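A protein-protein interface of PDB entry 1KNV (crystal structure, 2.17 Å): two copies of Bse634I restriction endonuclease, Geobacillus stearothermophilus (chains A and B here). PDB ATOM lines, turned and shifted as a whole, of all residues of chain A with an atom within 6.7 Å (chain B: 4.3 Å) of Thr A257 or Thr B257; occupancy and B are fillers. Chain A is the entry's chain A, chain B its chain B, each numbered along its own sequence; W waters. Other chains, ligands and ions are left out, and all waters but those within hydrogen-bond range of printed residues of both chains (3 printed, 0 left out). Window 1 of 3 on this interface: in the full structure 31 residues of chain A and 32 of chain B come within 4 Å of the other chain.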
ATOM      1  N   HIS A 211       4.341 -11.432 -12.470  1.00  0.00           N
ATOM      2  CA  HIS A 211       3.336 -12.174 -11.743  1.00  0.00           C
ATOM      3  C   HIS A 211       3.874 -12.874 -10.506  1.00  0.00           C
ATOM      4  O   HIS A 211       3.267 -12.814  -9.443  1.00  0.00           O
ATOM      5  CB  HIS A 211       2.675 -13.198 -12.659  1.00  0.00           C
ATOM      6  CG  HIS A 211       1.476 -13.843 -12.048  1.00  0.00           C
ATOM      7  ND1 HIS A 211       0.430 -13.116 -11.504  1.00  0.00           N
ATOM      8  CD2 HIS A 211       1.182 -15.140 -11.817  1.00  0.00           C
ATOM      9  CE1 HIS A 211      -0.440 -13.932 -10.960  1.00  0.00           C
ATOM     10  NE2 HIS A 211      -0.008 -15.176 -11.131  1.00  0.00           N
ATOM     11  N   ASN A 214       4.328 -10.633  -7.685  1.00  0.00           N
ATOM     12  CA  ASN A 214       3.041 -10.269  -7.114  1.00  0.00           C
ATOM     13  C   ASN A 214       2.545 -11.427  -6.252  1.00  0.00           C
ATOM     14  O   ASN A 214       2.053 -11.220  -5.147  1.00  0.00           O
ATOM     15  CB  ASN A 214       2.025  -9.975  -8.224  1.00  0.00           C
ATOM     16  CG  ASN A 214       1.983  -8.502  -8.607  1.00  0.00           C
ATOM     17  OD1 ASN A 214       1.556  -7.649  -7.815  1.00  0.00           O
ATOM     18  ND2 ASN A 214       2.431  -8.194  -9.824  1.00  0.00           N
ATOM     19  N   ILE A 215       2.691 -12.645  -6.768  1.00  0.00           N
ATOM     20  CA  ILE A 215       2.264 -13.850  -6.067  1.00  0.00           C
ATOM     21  C   ILE A 215       3.017 -14.072  -4.765  1.00  0.00           C
ATOM     22  O   ILE A 215       2.402 -14.289  -3.726  1.00  0.00           O
ATOM     23  CB  ILE A 215       2.436 -15.100  -6.959  1.00  0.00           C
ATOM     24  CG1 ILE A 215       1.370 -15.098  -8.051  1.00  0.00           C
ATOM     25  CG2 ILE A 215       2.314 -16.374  -6.134  1.00  0.00           C
ATOM     26  CD1 ILE A 215      -0.041 -15.318  -7.528  1.00  0.00           C
ATOM     27  N   LEU A 216       4.343 -14.025  -4.821  1.00  0.00           N
ATOM     28  CA  LEU A 216       5.162 -14.241  -3.631  1.00  0.00           C
ATOM     29  C   LEU A 216       5.084 -13.114  -2.613  1.00  0.00           C
ATOM     30  O   LEU A 216       4.988 -13.364  -1.405  1.00  0.00           O
ATOM     31  CB  LEU A 216       6.628 -14.463  -4.021  1.00  0.00           C
ATOM     32  CG  LEU A 216       6.871 -15.653  -4.958  1.00  0.00           C
ATOM     33  CD1 LEU A 216       8.360 -15.781  -5.288  1.00  0.00           C
ATOM     34  CD2 LEU A 216       6.353 -16.913  -4.296  1.00  0.00           C
ATOM     35  N   SER A 218       2.634 -10.906  -2.138  1.00  0.00           N
ATOM     36  CA  SER A 218       1.326 -10.784  -1.499  1.00  0.00           C
ATOM     37  C   SER A 218       1.195 -11.840  -0.396  1.00  0.00           C
ATOM     38  O   SER A 218       0.689 -11.562   0.700  1.00  0.00           O
ATOM     39  CB  SER A 218       0.200 -10.913  -2.537  1.00  0.00           C
ATOM     40  OG  SER A 218       0.211 -12.170  -3.185  1.00  0.00           O
ATOM     41  N   LEU A 219       1.673 -13.045  -0.685  1.00  0.00           N
ATOM     42  CA  LEU A 219       1.628 -14.129   0.278  1.00  0.00           C
ATOM     43  C   LEU A 219       2.421 -13.707   1.510  1.00  0.00           C
ATOM     44  O   LEU A 219       1.977 -13.887   2.639  1.00  0.00           O
ATOM     45  CB  LEU A 219       2.233 -15.391  -0.331  1.00  0.00           C
ATOM     46  CG  LEU A 219       2.124 -16.661   0.522  1.00  0.00           C
ATOM     47  CD1 LEU A 219       0.645 -17.005   0.731  1.00  0.00           C
ATOM     48  CD2 LEU A 219       2.821 -17.813  -0.161  1.00  0.00           C
ATOM     49  N   THR A 254       6.407  -1.781 -12.609  1.00  0.00           N
ATOM     50  CA  THR A 254       4.996  -1.985 -12.291  1.00  0.00           C
ATOM     51  C   THR A 254       4.784  -2.239 -10.799  1.00  0.00           C
ATOM     52  O   THR A 254       5.470  -3.056 -10.194  1.00  0.00           O
ATOM     53  CB  THR A 254       4.420  -3.155 -13.151  1.00  0.00           C
ATOM     54  OG1 THR A 254       3.063  -3.408 -12.778  1.00  0.00           O
ATOM     55  CG2 THR A 254       5.235  -4.424 -12.978  1.00  0.00           C
ATOM     56  N   ALA A 255       3.840  -1.518 -10.202  1.00  0.00           N
ATOM     57  CA  ALA A 255       3.534  -1.650  -8.778  1.00  0.00           C
ATOM     58  C   ALA A 255       2.877  -2.974  -8.405  1.00  0.00           C
ATOM     59  O   ALA A 255       2.027  -3.490  -9.138  1.00  0.00           O
ATOM     60  CB  ALA A 255       2.630  -0.499  -8.322  1.00  0.00           C
ATOM     61  N   ALA A 256       3.273  -3.514  -7.253  1.00  0.00           N
ATOM     62  CA  ALA A 256       2.701  -4.762  -6.763  1.00  0.00           C
ATOM     63  C   ALA A 256       1.255  -4.379  -6.488  1.00  0.00           C
ATOM     64  O   ALA A 256       0.998  -3.437  -5.736  1.00  0.00           O
ATOM     65  CB  ALA A 256       3.394  -5.187  -5.483  1.00  0.00           C
ATOM     66  N   THR A 257       0.318  -5.099  -7.102  1.00  0.00           N
ATOM     67  CA  THR A 257      -1.099  -4.779  -6.962  1.00  0.00           C
ATOM     68  C   THR A 257      -1.667  -4.757  -5.544  1.00  0.00           C
ATOM     69  O   THR A 257      -2.528  -3.929  -5.254  1.00  0.00           O
ATOM     70  CB  THR A 257      -1.976  -5.694  -7.872  1.00  0.00           C
ATOM     71  OG1 THR A 257      -1.716  -7.073  -7.586  1.00  0.00           O
ATOM     72  CG2 THR A 257      -1.661  -5.439  -9.340  1.00  0.00           C
ATOM     73  N   HIS A 258      -1.196  -5.630  -4.653  1.00  0.00           N
ATOM     74  CA  HIS A 258      -1.727  -5.641  -3.285  1.00  0.00           C
ATOM     75  C   HIS A 258      -1.240  -4.436  -2.510  1.00  0.00           C
ATOM     76  O   HIS A 258      -1.637  -4.216  -1.369  1.00  0.00           O
ATOM     77  CB  HIS A 258      -1.312  -6.909  -2.526  1.00  0.00           C
ATOM     78  CG  HIS A 258       0.133  -6.948  -2.135  1.00  0.00           C
ATOM     79  ND1 HIS A 258       1.125  -7.414  -2.980  1.00  0.00           N
ATOM     80  CD2 HIS A 258       0.761  -6.572  -1.000  1.00  0.00           C
ATOM     81  CE1 HIS A 258       2.293  -7.321  -2.378  1.00  0.00           C
ATOM     82  NE2 HIS A 258       2.102  -6.812  -1.172  1.00  0.00           N
ATOM     83  N   THR A 259      -0.393  -3.655  -3.163  1.00  0.00           N
ATOM     84  CA  THR A 259       0.230  -2.472  -2.590  1.00  0.00           C
ATOM     85  C   THR A 259      -0.542  -1.168  -2.798  1.00  0.00           C
ATOM     86  O   THR A 259      -0.331  -0.202  -2.064  1.00  0.00           O
ATOM     87  CB  THR A 259       1.661  -2.320  -3.176  1.00  0.00           C
ATOM     88  OG1 THR A 259       2.575  -3.132  -2.427  1.00  0.00           O
ATOM     89  CG2 THR A 259       2.111  -0.891  -3.162  1.00  0.00           C
ATOM     90  N   ILE A 260      -1.439  -1.139  -3.776  1.00  0.00           N
ATOM     91  CA  ILE A 260      -2.183   0.078  -4.055  1.00  0.00           C
ATOM     92  C   ILE A 260      -3.581   0.162  -3.446  1.00  0.00           C
ATOM     93  O   ILE A 260      -4.349   1.069  -3.778  1.00  0.00           O
ATOM     94  CB  ILE A 260      -2.312   0.309  -5.571  1.00  0.00           C
ATOM     95  CG1 ILE A 260      -3.131  -0.811  -6.209  1.00  0.00           C
ATOM     96  CG2 ILE A 260      -0.934   0.358  -6.205  1.00  0.00           C
ATOM     97  CD1 ILE A 260      -3.535  -0.493  -7.616  1.00  0.00           C
ATOM     98  N   VAL A 261      -3.927  -0.760  -2.555  1.00  0.00           N
ATOM     99  CA  VAL A 261      -5.254  -0.712  -1.972  1.00  0.00           C
ATOM    100  C   VAL A 261      -5.329  -0.058  -0.603  1.00  0.00           C
ATOM    101  O   VAL A 261      -6.362   0.481  -0.237  1.00  0.00           O
ATOM    102  CB  VAL A 261      -5.915  -2.101  -1.916  1.00  0.00           C
ATOM    103  CG1 VAL A 261      -6.284  -2.531  -3.326  1.00  0.00           C
ATOM    104  CG2 VAL A 261      -4.992  -3.114  -1.277  1.00  0.00           C
ATOM    105  N   GLU A 268       5.425  -0.494  -3.493  1.00  0.00           N
ATOM    106  CA  GLU A 268       6.575  -1.245  -3.976  1.00  0.00           C
ATOM    107  C   GLU A 268       6.350  -1.923  -5.318  1.00  0.00           C
ATOM    108  O   GLU A 268       5.214  -2.145  -5.738  1.00  0.00           O
ATOM    109  CB  GLU A 268       7.024  -2.284  -2.935  1.00  0.00           C
ATOM    110  CG  GLU A 268       6.042  -3.385  -2.639  1.00  0.00           C
ATOM    111  CD  GLU A 268       6.543  -4.338  -1.559  1.00  0.00           C
ATOM    112  OE1 GLU A 268       7.595  -4.983  -1.755  1.00  0.00           O
ATOM    113  OE2 GLU A 268       5.876  -4.443  -0.512  1.00  0.00           O
ATOM    114  N   ALA A 270       6.568  -5.015  -8.107  1.00  0.00           N
ATOM    115  CA  ALA A 270       6.300  -6.438  -8.042  1.00  0.00           C
ATOM    116  C   ALA A 270       7.698  -7.085  -8.048  1.00  0.00           C
ATOM    117  O   ALA A 270       7.940  -8.090  -7.375  1.00  0.00           O
ATOM    118  CB  ALA A 270       5.503  -6.868  -9.258  1.00  0.00           C
ATOM    119  N   ASN B 214      -5.626  -8.909 -12.321  1.00  0.00           N
ATOM    120  CA  ASN B 214      -5.076  -8.360 -11.083  1.00  0.00           C
ATOM    121  C   ASN B 214      -4.851  -6.867 -11.179  1.00  0.00           C
ATOM    122  O   ASN B 214      -5.146  -6.135 -10.238  1.00  0.00           O
ATOM    123  CB  ASN B 214      -3.757  -9.041 -10.734  1.00  0.00           C
ATOM    124  CG  ASN B 214      -3.962 -10.272  -9.902  1.00  0.00           C
ATOM    125  OD1 ASN B 214      -4.414 -10.183  -8.758  1.00  0.00           O
ATOM    126  ND2 ASN B 214      -3.648 -11.437 -10.468  1.00  0.00           N
ATOM    127  N   ILE B 215      -4.327  -6.429 -12.325  1.00  0.00           N
ATOM    128  CA  ILE B 215      -4.040  -5.012 -12.580  1.00  0.00           C
ATOM    129  C   ILE B 215      -5.303  -4.152 -12.580  1.00  0.00           C
ATOM    130  O   ILE B 215      -5.363  -3.118 -11.899  1.00  0.00           O
ATOM    131  CB  ILE B 215      -3.306  -4.818 -13.937  1.00  0.00           C
ATOM    132  CG1 ILE B 215      -1.861  -5.282 -13.812  1.00  0.00           C
ATOM    133  CG2 ILE B 215      -3.318  -3.350 -14.346  1.00  0.00           C
ATOM    134  CD1 ILE B 215      -1.037  -4.396 -12.886  1.00  0.00           C
ATOM    135  N   SER B 218      -7.415  -4.443  -9.051  1.00  0.00           N
ATOM    136  CA  SER B 218      -6.803  -3.717  -7.953  1.00  0.00           C
ATOM    137  C   SER B 218      -6.977  -2.212  -8.178  1.00  0.00           C
ATOM    138  O   SER B 218      -7.168  -1.446  -7.225  1.00  0.00           O
ATOM    139  CB  SER B 218      -5.325  -4.085  -7.827  1.00  0.00           C
ATOM    140  OG  SER B 218      -4.591  -3.738  -8.988  1.00  0.00           O
ATOM    141  N   ALA B 255      -6.516 -16.537  -6.919  1.00  0.00           N
ATOM    142  CA  ALA B 255      -7.040 -15.381  -6.201  1.00  0.00           C
ATOM    143  C   ALA B 255      -6.374 -14.045  -6.558  1.00  0.00           C
ATOM    144  O   ALA B 255      -5.159 -13.963  -6.713  1.00  0.00           O
ATOM    145  CB  ALA B 255      -6.911 -15.626  -4.711  1.00  0.00           C
ATOM    146  N   ALA B 256      -7.173 -12.994  -6.687  1.00  0.00           N
ATOM    147  CA  ALA B 256      -6.626 -11.678  -6.976  1.00  0.00           C
ATOM    148  C   ALA B 256      -5.694 -11.405  -5.796  1.00  0.00           C
ATOM    149  O   ALA B 256      -6.139 -11.415  -4.652  1.00  0.00           O
ATOM    150  CB  ALA B 256      -7.756 -10.657  -7.023  1.00  0.00           C
ATOM    151  N   THR B 257      -4.411 -11.173  -6.057  1.00  0.00           N
ATOM    152  CA  THR B 257      -3.455 -10.953  -4.972  1.00  0.00           C
ATOM    153  C   THR B 257      -3.768  -9.827  -3.990  1.00  0.00           C
ATOM    154  O   THR B 257      -3.401  -9.907  -2.809  1.00  0.00           O
ATOM    155  CB  THR B 257      -2.008 -10.738  -5.506  1.00  0.00           C
ATOM    156  OG1 THR B 257      -1.940  -9.535  -6.277  1.00  0.00           O
ATOM    157  CG2 THR B 257      -1.579 -11.907  -6.367  1.00  0.00           C
ATOM    158  N   HIS B 258      -4.438  -8.777  -4.450  1.00  0.00           N
ATOM    159  CA  HIS B 258      -4.748  -7.682  -3.539  1.00  0.00           C
ATOM    160  C   HIS B 258      -5.834  -8.055  -2.535  1.00  0.00           C
ATOM    161  O   HIS B 258      -6.039  -7.351  -1.543  1.00  0.00           O
ATOM    162  CB  HIS B 258      -5.152  -6.405  -4.306  1.00  0.00           C
ATOM    163  CG  HIS B 258      -6.481  -6.483  -4.987  1.00  0.00           C
ATOM    164  ND1 HIS B 258      -6.649  -7.023  -6.243  1.00  0.00           N
ATOM    165  CD2 HIS B 258      -7.720  -6.106  -4.573  1.00  0.00           C
ATOM    166  CE1 HIS B 258      -7.929  -6.979  -6.574  1.00  0.00           C
ATOM    167  NE2 HIS B 258      -8.600  -6.427  -5.577  1.00  0.00           N
ATOM    168  N   THR B 259      -6.516  -9.171  -2.767  1.00  0.00           N
ATOM    169  CA  THR B 259      -7.587  -9.562  -1.868  1.00  0.00           C
ATOM    170  C   THR B 259      -7.190 -10.505  -0.742  1.00  0.00           C
ATOM    171  O   THR B 259      -8.048 -10.890   0.050  1.00  0.00           O
ATOM    172  CB  THR B 259      -8.767 -10.206  -2.637  1.00  0.00           C
ATOM    173  OG1 THR B 259      -8.367 -11.466  -3.187  1.00  0.00           O
ATOM    174  CG2 THR B 259      -9.231  -9.291  -3.765  1.00  0.00           C
ATOM    175  N   ILE B 260      -5.913 -10.882  -0.649  1.00  0.00           N
ATOM    176  CA  ILE B 260      -5.511 -11.798   0.421  1.00  0.00           C
ATOM    177  C   ILE B 260      -4.723 -11.161   1.557  1.00  0.00           C
ATOM    178  O   ILE B 260      -4.160 -11.869   2.394  1.00  0.00           O
ATOM    179  CB  ILE B 260      -4.683 -13.011  -0.101  1.00  0.00           C
ATOM    180  CG1 ILE B 260      -3.318 -12.555  -0.624  1.00  0.00           C
ATOM    181  CG2 ILE B 260      -5.458 -13.745  -1.184  1.00  0.00           C
ATOM    182  CD1 ILE B 260      -2.386 -13.729  -0.965  1.00  0.00           C
HETATM  183  O   HOH W   1      -0.945  -9.328  -9.099  1.00  0.00           O
HETATM  184  O   HOH W   2       0.268  -8.063  -5.280  1.00  0.00           O
HETATM  185  O   HOH W   3      -4.497  -7.893  -7.367  1.00  0.00           O
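Ile A215 touches Thr B257, and with the chains exchanged Thr A257 touches Ile B215. Ser A218 touches Thr B257, and with the chains exchanged Thr A257 touches Ser B218. Thr A257 touches His B258, and with the chains exchanged His A258 touches Thr B257. His B258 touches its own counterpart, His A258. Of the 12 pairs that touch across the chains among the printed residues, 12 have their exchanged pair printed and touching as well.
Printed residues of chain B that touch a printed residue of chain A: Asn B214, Ile B215, Ser B218, Thr B257, His B258 and Ile B260. Hydrophobic or aromatic side chains of chain B that line the printed part of chain A: Ile B215, His B258 and Ile B260. Of the 16 printed residues of chain A, 6 touch a printed residue of chain B. Printed residues of chain A that touch a printed residue of chain B: Asn A214, Ile A215, Ser A218, Thr A257, His A258 and Ile A260. Hydrophobic or aromatic side chains of chain A that line the printed part of chain B: Ile A215, His A258 and Ile A260. Among the printed residues, 12 pairs touch across the chains.
Of chain B, only Asn B214, Ile B215, Ser B218, Thr B257 and His B258 come within 4 Å of Thr A257. Of chain A, only Asn A214, Ile A215, Ser A218, Thr A257 and His A258 come within 4 Å of Thr B257. Of the printed residues of chain A, Ile B260 touches Ser A218. Of the printed residues of chain A, Ser B218 touches Thr A257 and Ile A260. Thr A259 touches none of the printed residues of chain B.
The backbone carbonyl oxygen (O) of Asn A214 lies within hydrogen-bond range of the side-chain hydroxyl (OG) of Ser A218. The side-chain amide oxygen of Asn A214 sits at hydrogen-bond distance from the backbone NH of Thr A257, 2.9 Å away. O of Ile A215 is in hydrogen-bond range of OG of Ser A218, at 3.1 Å. O of Asn B214 sits at hydrogen-bond distance from OG of Ser B218, 2.8 Å away. The side-chain amide oxygen (OD1) of Asn B214 lies within hydrogen-bond range of the backbone NH (N) of Thr B257, at 2.9 Å. The side-chain hydroxyl of Ser B218 is in hydrogen-bond range of the backbone carbonyl oxygen of Ile B215 (3.1 Å).
Water W2 lies within hydrogen-bond range of a ring nitrogen (ND1) of His A258, the side-chain hydroxyl (OG1) of Thr B257, the side-chain amide oxygen (OD1) of Asn A214 and the side-chain hydroxyl (OG1) of Thr A257. Water W3 lies within hydrogen-bond range of a ring nitrogen (ND1) of His B258 (2.6 Å), the side-chain amide oxygen (OD1) of Asn B214 (2.7 Å), the side-chain hydroxyl (OG1) of Thr A257 (2.9 Å) and the side-chain hydroxyl (OG1) of Thr B257 (3.2 Å). Water W1 lies within hydrogen-bond range of the side-chain hydroxyl of Thr A257 (2.8 Å), the side-chain hydroxyl of Thr B257 (3.0 Å) and the side-chain amide oxygen of Asn A214 (3.3 Å).
Thr B257 touches Ile A215. Ser A218 touches Thr B257. Ile B260 touches Ser A218 (CD1 to OG, 3.8 Å). Thr A257 touches Asn B214. Ile B215 touches Thr A257. OG of Ser B218 touches CG2 of Thr A257, at 3.4 Å. O of Thr A257 touches CB of His B258, 3.7 Å away. His A258 touches Thr B257. His A258 touches His B258. OG of Ser B218 touches CD1 of Ile A260, at 3.7 Å.
The side-chain hydroxyl (OG1) of Thr A257 lies within hydrogen-bond range of the side-chain hydroxyl (OG1) of Thr B257 (2.8 Å).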
